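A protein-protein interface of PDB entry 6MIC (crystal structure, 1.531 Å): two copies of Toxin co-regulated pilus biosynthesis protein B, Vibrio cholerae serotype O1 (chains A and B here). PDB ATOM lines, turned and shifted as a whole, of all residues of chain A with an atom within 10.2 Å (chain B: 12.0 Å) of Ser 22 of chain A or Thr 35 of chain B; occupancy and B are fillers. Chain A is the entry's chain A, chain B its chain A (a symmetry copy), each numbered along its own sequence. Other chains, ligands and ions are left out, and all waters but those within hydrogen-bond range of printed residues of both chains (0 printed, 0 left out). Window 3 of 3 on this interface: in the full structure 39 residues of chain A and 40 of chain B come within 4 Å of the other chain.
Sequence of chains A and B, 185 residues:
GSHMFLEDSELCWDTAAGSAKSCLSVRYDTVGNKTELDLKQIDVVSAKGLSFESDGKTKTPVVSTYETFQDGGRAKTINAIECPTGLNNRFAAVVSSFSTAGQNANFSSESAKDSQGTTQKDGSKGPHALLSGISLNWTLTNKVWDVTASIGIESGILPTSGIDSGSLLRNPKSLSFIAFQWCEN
The backbone NH (N) of Val 44 of chain A sits at hydrogen-bond distance from the backbone carbonyl oxygen (O) of Thr 35 of chain B (3.2 Å). The side-chain carboxylate (OD2) of Asp 43 of chain A sits at hydrogen-bond distance from the backbone NH (N) of Thr 35 of chain B (2.8 Å). The backbone carbonyl oxygen (O) of Val 44 of chain A is in hydrogen-bond range of the backbone NH (N) of Leu 37 of chain B. The backbone carbonyl oxygen (O) of Leu 37 of chain B lies within hydrogen-bond range of the backbone NH (N) of Ser 46 of chain A (3.0 Å). The backbone NH (N) of Leu 39 of chain B lies within hydrogen-bond range of the backbone carbonyl oxygen (O) of Ser 46 of chain A. The side-chain amino group (NZ) of Lys 40 of chain B sits at hydrogen-bond distance from the side-chain hydroxyl (OG) of Ser 46 of chain A.
The backbone carbonyl oxygen (O) of Glu 36 of chain B sits at hydrogen-bond distance from the backbone NH (N) of Arg 27 of chain B (2.9 Å). The backbone carbonyl oxygen (O) of Ser 25 of chain B sits at hydrogen-bond distance from the backbone NH (N) of Asp 38 of chain B (3.0 Å). OD2 of Asp 38 of chain B is in salt-bridge range of NZ of Lys 40 of chain B (2.9 Å). The side-chain carboxylate (OD2) of Asp 38 of chain A lies within salt-bridge range of the side-chain amino group (NZ) of Lys 40 of chain A (2.9 Å). The side-chain carboxylate (OE2) of Glu 36 of chain B is in salt-bridge range of the side-chain amino group (NZ) of Lys 40 of chain B (3.6 Å). The backbone carbonyl oxygen (O) of Ser 22 of chain A sits close to the side-chain amide oxygen (OE1) of Gln 41 of chain A (2.9 Å).
CD2 of Leu 39 of chain A touches CD1 of Leu 37 of chain B (3.9 Å). Lys 40 of chain A touches Glu 53 of chain B. OG1 of Thr 35 of chain B touches CG2 of Ile 42 of chain A, at 3.5 Å. Ile 42 of chain A touches Glu 36 of chain B (CG2 to N, 3.6 Å). CG2 of Ile 42 of chain A touches N of Leu 37 of chain B, at 3.5 Å. OD2 of Asp 43 of chain A touches CA of Lys 34 of chain B, 3.3 Å away. Glu 36 of chain B touches Val 44 of chain A. Val 45 of chain A touches Leu 39 of chain B. Glu 36 of chain B touches Ser 46 of chain A (OE2 to CB, 3.6 Å). Asp 38 of chain B touches Ser 46 of chain A.
No residue of chain B comes within 4 Å of Cys 23 of chain A. No residue of chain B comes within 4 Å of Gln 41 of chain A. Ile 42 of chain A touches just these residues of chain B: Thr 35, Glu 36 and Leu 37. Asp 43 of chain A touches just these residues of chain B: Lys 34 (3.3 Å) and Thr 35 (2.8 Å). Of chain B, only Thr 35 (3.2 Å), Glu 36 (3.2 Å) and Leu 37 (2.8 Å) come within 4 Å of Val 44 of chain A. Of the printed residues of chain B, Val 45 of chain A touches Leu 37 and Leu 39. Of the printed residues of chain B, Ser 46 of chain A touches Glu 36 (3.6 Å), Leu 37 (3.0 Å), Asp 38 (3.9 Å), Leu 39 (2.8 Å) and Lys 40 (3.0 Å). Leu 24 of chain B touches none of the printed residues of chain A. Of the printed residues of chain A, Lys 34 of chain B touches Asp 43 (3.3 Å). Of chain A, only Ser 22, Ile 42, Asp 43 and Val 44 come within 4 Å of Thr 35 of chain B. Of the printed residues of chain A, Asp 38 of chain B touches Ser 46 (3.9 Å). The nearest residue of chain B that does not touch Ser 22 of chain A is Val 26 of chain B (4.9 Å). The nearest residue of chain A that does not touch Thr 35 of chain B is Gln 41 of chain A (4.2 Å).
Of the 18 printed residues of chain B, 8 touch a printed residue of chain A. Hydrophobic or aromatic side chains of chain B within 4 Å of the printed part of chain A: Leu 37 and Leu 39.
5 positions are printed for both chains.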
ATOM      1  N   SER A  22      22.279  -6.169  30.050  1.00  0.00           N
ATOM      2  CA  SER A  22      21.505  -6.049  28.819  1.00  0.00           C
ATOM      3  C   SER A  22      22.416  -6.062  27.587  1.00  0.00           C
ATOM      4  O   SER A  22      22.333  -6.967  26.755  1.00  0.00           O
ATOM      5  CB  SER A  22      20.665  -4.769  28.842  1.00  0.00           C
ATOM      6  OG  SER A  22      19.693  -4.814  29.874  1.00  0.00           O
ATOM      7  N   CYS A  23      23.275  -5.048  27.476  1.00  0.00           N
ATOM      8  CA  CYS A  23      24.247  -4.959  26.388  1.00  0.00           C
ATOM      9  C   CYS A  23      23.572  -4.763  25.033  1.00  0.00           C
ATOM     10  O   CYS A  23      22.341  -4.778  24.933  1.00  0.00           O
ATOM     11  CB  CYS A  23      25.132  -6.209  26.359  1.00  0.00           C
ATOM     12  SG  CYS A  23      26.628  -6.034  25.349  1.00  0.00           S
ATOM     13  N   LEU A  24      24.377  -4.582  23.988  1.00  0.00           N
ATOM     14  CA  LEU A  24      23.878  -4.312  22.645  1.00  0.00           C
ATOM     15  C   LEU A  24      24.977  -4.659  21.654  1.00  0.00           C
ATOM     16  O   LEU A  24      26.137  -4.841  22.026  1.00  0.00           O
ATOM     17  CB  LEU A  24      23.433  -2.849  22.490  1.00  0.00           C
ATOM     18  CG  LEU A  24      24.468  -1.707  22.515  1.00  0.00           C
ATOM     19  CD1 LEU A  24      25.427  -1.818  23.690  1.00  0.00           C
ATOM     20  CD2 LEU A  24      25.250  -1.570  21.206  1.00  0.00           C
ATOM     21  N   SER A  25      24.605  -4.732  20.378  1.00  0.00           N
ATOM     22  CA  SER A  25      25.564  -5.097  19.345  1.00  0.00           C
ATOM     23  C   SER A  25      24.993  -4.770  17.973  1.00  0.00           C
ATOM     24  O   SER A  25      23.799  -4.498  17.816  1.00  0.00           O
ATOM     25  CB  SER A  25      25.926  -6.581  19.430  1.00  0.00           C
ATOM     26  OG  SER A  25      24.766  -7.389  19.301  1.00  0.00           O
ATOM     27  N   ASP A  38      21.125  -3.450  17.026  1.00  0.00           N
ATOM     28  CA  ASP A  38      20.102  -4.034  17.880  1.00  0.00           C
ATOM     29  C   ASP A  38      20.151  -3.375  19.253  1.00  0.00           C
ATOM     30  O   ASP A  38      21.167  -3.454  19.952  1.00  0.00           O
ATOM     31  CB  ASP A  38      20.297  -5.545  18.001  1.00  0.00           C
ATOM     32  CG  ASP A  38      19.160  -6.220  18.729  1.00  0.00           C
ATOM     33  OD1 ASP A  38      19.392  -7.293  19.322  1.00  0.00           O
ATOM     34  OD2 ASP A  38      18.035  -5.679  18.711  1.00  0.00           O
ATOM     35  N   LEU A  39      19.054  -2.721  19.632  1.00  0.00           N
ATOM     36  CA  LEU A  39      18.909  -2.120  20.951  1.00  0.00           C
ATOM     37  C   LEU A  39      17.719  -2.708  21.695  1.00  0.00           C
ATOM     38  O   LEU A  39      17.364  -2.211  22.771  1.00  0.00           O
ATOM     39  CB  LEU A  39      18.776  -0.597  20.819  1.00  0.00           C
ATOM     40  CG  LEU A  39      19.939   0.043  20.060  1.00  0.00           C
ATOM     41  CD1 LEU A  39      19.695   1.512  19.773  1.00  0.00           C
ATOM     42  CD2 LEU A  39      21.235  -0.132  20.846  1.00  0.00           C
ATOM     43  N   LYS A  40      17.106  -3.763  21.148  1.00  0.00           N
ATOM     44  CA  LYS A  40      15.880  -4.338  21.672  1.00  0.00           C
ATOM     45  C   LYS A  40      16.093  -5.062  22.993  1.00  0.00           C
ATOM     46  O   LYS A  40      15.106  -5.429  23.640  1.00  0.00           O
ATOM     47  CB  LYS A  40      15.278  -5.295  20.637  1.00  0.00           C
ATOM     48  CG  LYS A  40      14.822  -4.613  19.339  1.00  0.00           C
ATOM     49  CD  LYS A  40      13.971  -5.536  18.476  1.00  0.00           C
ATOM     50  CE  LYS A  40      14.783  -6.663  17.860  1.00  0.00           C
ATOM     51  NZ  LYS A  40      15.791  -6.178  16.889  1.00  0.00           N
ATOM     52  N   GLN A  41      17.345  -5.282  23.395  1.00  0.00           N
ATOM     53  CA  GLN A  41      17.610  -5.857  24.706  1.00  0.00           C
ATOM     54  C   GLN A  41      17.353  -4.845  25.818  1.00  0.00           C
ATOM     55  O   GLN A  41      17.035  -5.237  26.947  1.00  0.00           O
ATOM     56  CB  GLN A  41      19.048  -6.381  24.759  1.00  0.00           C
ATOM     57  CG  GLN A  41      19.361  -7.443  23.698  1.00  0.00           C
ATOM     58  CD  GLN A  41      20.701  -8.131  23.919  1.00  0.00           C
ATOM     59  OE1 GLN A  41      20.938  -8.728  24.971  1.00  0.00           O
ATOM     60  NE2 GLN A  41      21.585  -8.048  22.928  1.00  0.00           N
ATOM     61  N   ILE A  42      17.473  -3.541  25.517  1.00  0.00           N
ATOM     62  CA  ILE A  42      17.136  -2.470  26.454  1.00  0.00           C
ATOM     63  C   ILE A  42      15.675  -2.077  26.251  1.00  0.00           C
ATOM     64  O   ILE A  42      15.173  -2.072  25.123  1.00  0.00           O
ATOM     65  CB  ILE A  42      18.082  -1.268  26.261  1.00  0.00           C
ATOM     66  CG1 ILE A  42      19.552  -1.706  26.342  1.00  0.00           C
ATOM     67  CG2 ILE A  42      17.824  -0.208  27.314  1.00  0.00           C
ATOM     68  CD1 ILE A  42      20.213  -1.944  25.002  1.00  0.00           C
ATOM     69  N   ASP A  43      14.980  -1.740  27.347  1.00  0.00           N
ATOM     70  CA  ASP A  43      13.536  -1.514  27.274  1.00  0.00           C
ATOM     71  C   ASP A  43      13.178  -0.158  26.667  1.00  0.00           C
ATOM     72  O   ASP A  43      12.147  -0.043  25.990  1.00  0.00           O
ATOM     73  CB  ASP A  43      12.905  -1.625  28.665  1.00  0.00           C
ATOM     74  CG  ASP A  43      13.002  -3.028  29.244  1.00  0.00           C
ATOM     75  OD1 ASP A  43      12.227  -3.909  28.815  1.00  0.00           O
ATOM     76  OD2 ASP A  43      13.854  -3.250  30.132  1.00  0.00           O
ATOM     77  N   VAL A  44      13.976   0.877  26.920  1.00  0.00           N
ATOM     78  CA  VAL A  44      13.734   2.209  26.373  1.00  0.00           C
ATOM     79  C   VAL A  44      15.063   2.793  25.922  1.00  0.00           C
ATOM     80  O   VAL A  44      16.082   2.648  26.605  1.00  0.00           O
ATOM     81  CB  VAL A  44      13.048   3.144  27.396  1.00  0.00           C
ATOM     82  CG1 VAL A  44      12.837   4.536  26.803  1.00  0.00           C
ATOM     83  CG2 VAL A  44      11.725   2.553  27.854  1.00  0.00           C
ATOM     84  N   VAL A  45      15.046   3.450  24.764  1.00  0.00           N
ATOM     85  CA  VAL A  45      16.155   4.253  24.265  1.00  0.00           C
ATOM     86  C   VAL A  45      15.731   5.706  24.427  1.00  0.00           C
ATOM     87  O   VAL A  45      14.695   6.115  23.890  1.00  0.00           O
ATOM     88  CB  VAL A  45      16.477   3.920  22.798  1.00  0.00           C
ATOM     89  CG1 VAL A  45      17.555   4.837  22.246  1.00  0.00           C
ATOM     90  CG2 VAL A  45      16.886   2.461  22.676  1.00  0.00           C
ATOM     91  N   SER A  46      16.494   6.479  25.198  1.00  0.00           N
ATOM     92  CA  SER A  46      16.145   7.855  25.525  1.00  0.00           C
ATOM     93  C   SER A  46      17.147   8.797  24.871  1.00  0.00           C
ATOM     94  O   SER A  46      18.333   8.776  25.210  1.00  0.00           O
ATOM     95  CB  SER A  46      16.124   8.062  27.042  1.00  0.00           C
ATOM     96  OG  SER A  46      16.017   9.427  27.361  1.00  0.00           O
ATOM     97  N   LEU B  24      28.042   7.978  27.048  1.00  0.00           N
ATOM     98  CA  LEU B  24      26.698   7.436  27.197  1.00  0.00           C
ATOM     99  C   LEU B  24      26.793   6.154  28.009  1.00  0.00           C
ATOM    100  O   LEU B  24      27.876   5.600  28.203  1.00  0.00           O
ATOM    101  CB  LEU B  24      26.035   7.181  25.834  1.00  0.00           C
ATOM    102  CG  LEU B  24      26.559   6.069  24.902  1.00  0.00           C
ATOM    103  CD1 LEU B  24      28.068   6.125  24.725  1.00  0.00           C
ATOM    104  CD2 LEU B  24      26.129   4.664  25.334  1.00  0.00           C
ATOM    105  N   SER B  25      25.640   5.674  28.472  1.00  0.00           N
ATOM    106  CA  SER B  25      25.614   4.474  29.296  1.00  0.00           C
ATOM    107  C   SER B  25      24.189   3.946  29.394  1.00  0.00           C
ATOM    108  O   SER B  25      23.222   4.625  29.037  1.00  0.00           O
ATOM    109  CB  SER B  25      26.173   4.754  30.693  1.00  0.00           C
ATOM    110  OG  SER B  25      25.433   5.781  31.333  1.00  0.00           O
ATOM    111  N   VAL B  26      24.080   2.721  29.898  1.00  0.00           N
ATOM    112  CA  VAL B  26      22.802   2.051  30.117  1.00  0.00           C
ATOM    113  C   VAL B  26      22.463   2.172  31.599  1.00  0.00           C
ATOM    114  O   VAL B  26      23.091   1.525  32.443  1.00  0.00           O
ATOM    115  CB  VAL B  26      22.858   0.580  29.681  1.00  0.00           C
ATOM    116  CG1 VAL B  26      21.481  -0.064  29.783  1.00  0.00           C
ATOM    117  CG2 VAL B  26      23.417   0.452  28.262  1.00  0.00           C
ATOM    118  N   ARG B  27      21.466   2.989  31.925  1.00  0.00           N
ATOM    119  CA  ARG B  27      21.053   3.191  33.305  1.00  0.00           C
ATOM    120  C   ARG B  27      19.812   2.350  33.605  1.00  0.00           C
ATOM    121  O   ARG B  27      19.259   1.679  32.731  1.00  0.00           O
ATOM    122  CB  ARG B  27      20.808   4.678  33.574  1.00  0.00           C
ATOM    123  CG  ARG B  27      21.822   5.592  32.894  1.00  0.00           C
ATOM    124  CD  ARG B  27      22.036   6.905  33.629  1.00  0.00           C
ATOM    125  NE  ARG B  27      20.804   7.473  34.169  1.00  0.00           N
ATOM    126  CZ  ARG B  27      20.449   7.455  35.453  1.00  0.00           C
ATOM    127  NH1 ARG B  27      19.306   8.011  35.823  1.00  0.00           N
ATOM    128  NH2 ARG B  27      21.225   6.890  36.369  1.00  0.00           N
ATOM    129  N   TYR B  28      19.375   2.383  34.863  1.00  0.00           N
ATOM    130  CA  TYR B  28      18.222   1.602  35.300  1.00  0.00           C
ATOM    131  C   TYR B  28      17.496   2.347  36.409  1.00  0.00           C
ATOM    132  O   TYR B  28      18.127   2.786  37.375  1.00  0.00           O
ATOM    133  CB  TYR B  28      18.648   0.217  35.799  1.00  0.00           C
ATOM    134  CG  TYR B  28      17.522  -0.561  36.447  1.00  0.00           C
ATOM    135  CD1 TYR B  28      16.566  -1.210  35.678  1.00  0.00           C
ATOM    136  CD2 TYR B  28      17.415  -0.641  37.831  1.00  0.00           C
ATOM    137  CE1 TYR B  28      15.533  -1.919  36.269  1.00  0.00           C
ATOM    138  CE2 TYR B  28      16.387  -1.349  38.429  1.00  0.00           C
ATOM    139  CZ  TYR B  28      15.451  -1.984  37.642  1.00  0.00           C
ATOM    140  OH  TYR B  28      14.428  -2.688  38.234  1.00  0.00           O
ATOM    141  N   ASP B  29      16.178   2.478  36.276  1.00  0.00           N
ATOM    142  CA  ASP B  29      15.358   3.146  37.277  1.00  0.00           C
ATOM    143  C   ASP B  29      14.558   2.130  38.080  1.00  0.00           C
ATOM    144  O   ASP B  29      14.102   1.108  37.554  1.00  0.00           O
ATOM    145  CB  ASP B  29      14.400   4.165  36.642  1.00  0.00           C
ATOM    146  CG  ASP B  29      13.434   3.533  35.649  1.00  0.00           C
ATOM    147  OD1 ASP B  29      13.572   3.799  34.435  1.00  0.00           O
ATOM    148  OD2 ASP B  29      12.532   2.781  36.078  1.00  0.00           O
ATOM    149  N   THR B  30      14.387   2.436  39.368  1.00  0.00           N
ATOM    150  CA  THR B  30      13.668   1.553  40.277  1.00  0.00           C
ATOM    151  C   THR B  30      12.163   1.574  40.042  1.00  0.00           C
ATOM    152  O   THR B  30      11.476   0.614  40.406  1.00  0.00           O
ATOM    153  CB  THR B  30      13.970   1.947  41.725  1.00  0.00           C
ATOM    154  OG1 THR B  30      13.632   3.324  41.928  1.00  0.00           O
ATOM    155  CG2 THR B  30      15.446   1.737  42.043  1.00  0.00           C
ATOM    156  N   VAL B  31      11.636   2.644  39.445  1.00  0.00           N
ATOM    157  CA  VAL B  31      10.208   2.741  39.162  1.00  0.00           C
ATOM    158  C   VAL B  31       9.857   1.702  38.107  1.00  0.00           C
ATOM    159  O   VAL B  31      10.006   1.944  36.905  1.00  0.00           O
ATOM    160  CB  VAL B  31       9.824   4.159  38.700  1.00  0.00           C
ATOM    161  CG1 VAL B  31       8.342   4.232  38.350  1.00  0.00           C
ATOM    162  CG2 VAL B  31      10.168   5.179  39.778  1.00  0.00           C
ATOM    163  N   GLY B  32       9.389   0.539  38.555  1.00  0.00           N
ATOM    164  CA  GLY B  32       9.068  -0.554  37.658  1.00  0.00           C
ATOM    165  C   GLY B  32      10.178  -1.581  37.602  1.00  0.00           C
ATOM    166  O   GLY B  32      10.811  -1.876  38.620  1.00  0.00           O
ATOM    167  N   ASN B  33      10.420  -2.142  36.423  1.00  0.00           N
ATOM    168  CA  ASN B  33      11.501  -3.101  36.233  1.00  0.00           C
ATOM    169  C   ASN B  33      11.922  -3.072  34.765  1.00  0.00           C
ATOM    170  O   ASN B  33      11.806  -4.051  34.031  1.00  0.00           O
ATOM    171  CB  ASN B  33      11.074  -4.499  36.675  1.00  0.00           C
ATOM    172  CG  ASN B  33      12.214  -5.499  36.621  1.00  0.00           C
ATOM    173  OD1 ASN B  33      13.387  -5.118  36.595  1.00  0.00           O
ATOM    174  ND2 ASN B  33      11.876  -6.782  36.600  1.00  0.00           N
ATOM    175  N   LYS B  34      12.431  -1.921  34.323  1.00  0.00           N
ATOM    176  CA  LYS B  34      12.810  -1.739  32.931  1.00  0.00           C
ATOM    177  C   LYS B  34      14.108  -0.945  32.852  1.00  0.00           C
ATOM    178  O   LYS B  34      14.366  -0.065  33.678  1.00  0.00           O
ATOM    179  CB  LYS B  34      11.686  -1.033  32.148  1.00  0.00           C
ATOM    180  CG  LYS B  34      10.495  -1.944  31.820  1.00  0.00           C
ATOM    181  CD  LYS B  34       9.304  -1.152  31.293  1.00  0.00           C
ATOM    182  CE  LYS B  34       8.191  -2.068  30.790  1.00  0.00           C
ATOM    183  NZ  LYS B  34       6.958  -1.310  30.420  1.00  0.00           N
ATOM    184  N   THR B  35      14.935  -1.287  31.866  1.00  0.00           N
ATOM    185  CA  THR B  35      16.213  -0.631  31.642  1.00  0.00           C
ATOM    186  C   THR B  35      16.065   0.511  30.635  1.00  0.00           C
ATOM    187  O   THR B  35      15.045   0.652  29.959  1.00  0.00           O
ATOM    188  CB  THR B  35      17.244  -1.635  31.134  1.00  0.00           C
ATOM    189  OG1 THR B  35      16.748  -2.266  29.948  1.00  0.00           O
ATOM    190  CG2 THR B  35      17.536  -2.700  32.187  1.00  0.00           C
ATOM    191  N   GLU B  36      17.119   1.314  30.516  1.00  0.00           N
ATOM    192  CA  GLU B  36      17.058   2.489  29.660  1.00  0.00           C
ATOM    193  C   GLU B  36      18.453   2.856  29.173  1.00  0.00           C
ATOM    194  O   GLU B  36      19.402   2.891  29.958  1.00  0.00           O
ATOM    195  CB  GLU B  36      16.436   3.672  30.403  1.00  0.00           C
ATOM    196  CG  GLU B  36      16.323   4.925  29.564  1.00  0.00           C
ATOM    197  CD  GLU B  36      15.608   6.047  30.291  1.00  0.00           C
ATOM    198  OE1 GLU B  36      14.424   5.869  30.653  1.00  0.00           O
ATOM    199  OE2 GLU B  36      16.238   7.105  30.508  1.00  0.00           O
ATOM    200  N   LEU B  37      18.561   3.152  27.880  1.00  0.00           N
ATOM    201  CA  LEU B  37      19.819   3.573  27.274  1.00  0.00           C
ATOM    202  C   LEU B  37      19.819   5.092  27.182  1.00  0.00           C
ATOM    203  O   LEU B  37      19.078   5.675  26.381  1.00  0.00           O
ATOM    204  CB  LEU B  37      20.001   2.940  25.899  1.00  0.00           C
ATOM    205  CG  LEU B  37      21.443   2.749  25.425  1.00  0.00           C
ATOM    206  CD1 LEU B  37      21.448   2.123  24.045  1.00  0.00           C
ATOM    207  CD2 LEU B  37      22.209   4.056  25.421  1.00  0.00           C
ATOM    208  N   ASP B  38      20.665   5.733  27.984  1.00  0.00           N
ATOM    209  CA  ASP B  38      20.682   7.185  28.093  1.00  0.00           C
ATOM    210  C   ASP B  38      21.585   7.765  27.011  1.00  0.00           C
ATOM    211  O   ASP B  38      22.787   7.479  26.977  1.00  0.00           O
ATOM    212  CB  ASP B  38      21.160   7.615  29.480  1.00  0.00           C
ATOM    213  CG  ASP B  38      21.024   9.103  29.702  1.00  0.00           C
ATOM    214  OD1 ASP B  38      21.789   9.649  30.524  1.00  0.00           O
ATOM    215  OD2 ASP B  38      20.157   9.726  29.057  1.00  0.00           O
ATOM    216  N   LEU B  39      21.001   8.572  26.127  1.00  0.00           N
ATOM    217  CA  LEU B  39      21.744   9.278  25.092  1.00  0.00           C
ATOM    218  C   LEU B  39      21.570  10.783  25.221  1.00  0.00           C
ATOM    219  O   LEU B  39      22.013  11.528  24.339  1.00  0.00           O
ATOM    220  CB  LEU B  39      21.299   8.791  23.706  1.00  0.00           C
ATOM    221  CG  LEU B  39      21.435   7.278  23.529  1.00  0.00           C
ATOM    222  CD1 LEU B  39      20.814   6.794  22.234  1.00  0.00           C
ATOM    223  CD2 LEU B  39      22.905   6.875  23.592  1.00  0.00           C
ATOM    224  N   LYS B  40      20.943  11.243  26.309  1.00  0.00           N
ATOM    225  CA  LYS B  40      20.585  12.638  26.498  1.00  0.00           C
ATOM    226  C   LYS B  40      21.797  13.525  26.740  1.00  0.00           C
ATOM    227  O   LYS B  40      21.654  14.751  26.723  1.00  0.00           O
ATOM    228  CB  LYS B  40      19.600  12.761  27.666  1.00  0.00           C
ATOM    229  CG  LYS B  40      18.246  12.078  27.423  1.00  0.00           C
ATOM    230  CD  LYS B  40      17.210  12.475  28.467  1.00  0.00           C
ATOM    231  CE  LYS B  40      17.512  11.887  29.835  1.00  0.00           C
ATOM    232  NZ  LYS B  40      17.417  10.409  29.856  1.00  0.00           N
ATOM    233  N   GLU B  53       9.381  -0.175  18.877  1.00  0.00           N
ATOM    234  CA  GLU B  53       8.234  -1.005  19.186  1.00  0.00           C
ATOM    235  C   GLU B  53       7.176  -0.203  19.919  1.00  0.00           C
ATOM    236  O   GLU B  53       7.486   0.675  20.734  1.00  0.00           O
ATOM    237  CB  GLU B  53       8.633  -2.232  19.993  1.00  0.00           C
ATOM    238  CG  GLU B  53       9.576  -3.142  19.207  1.00  0.00           C
ATOM    239  CD  GLU B  53       9.907  -4.462  19.886  1.00  0.00           C
ATOM    240  OE1 GLU B  53       9.281  -4.781  20.921  1.00  0.00           O
ATOM    241  OE2 GLU B  53      10.786  -5.185  19.353  1.00  0.00           O
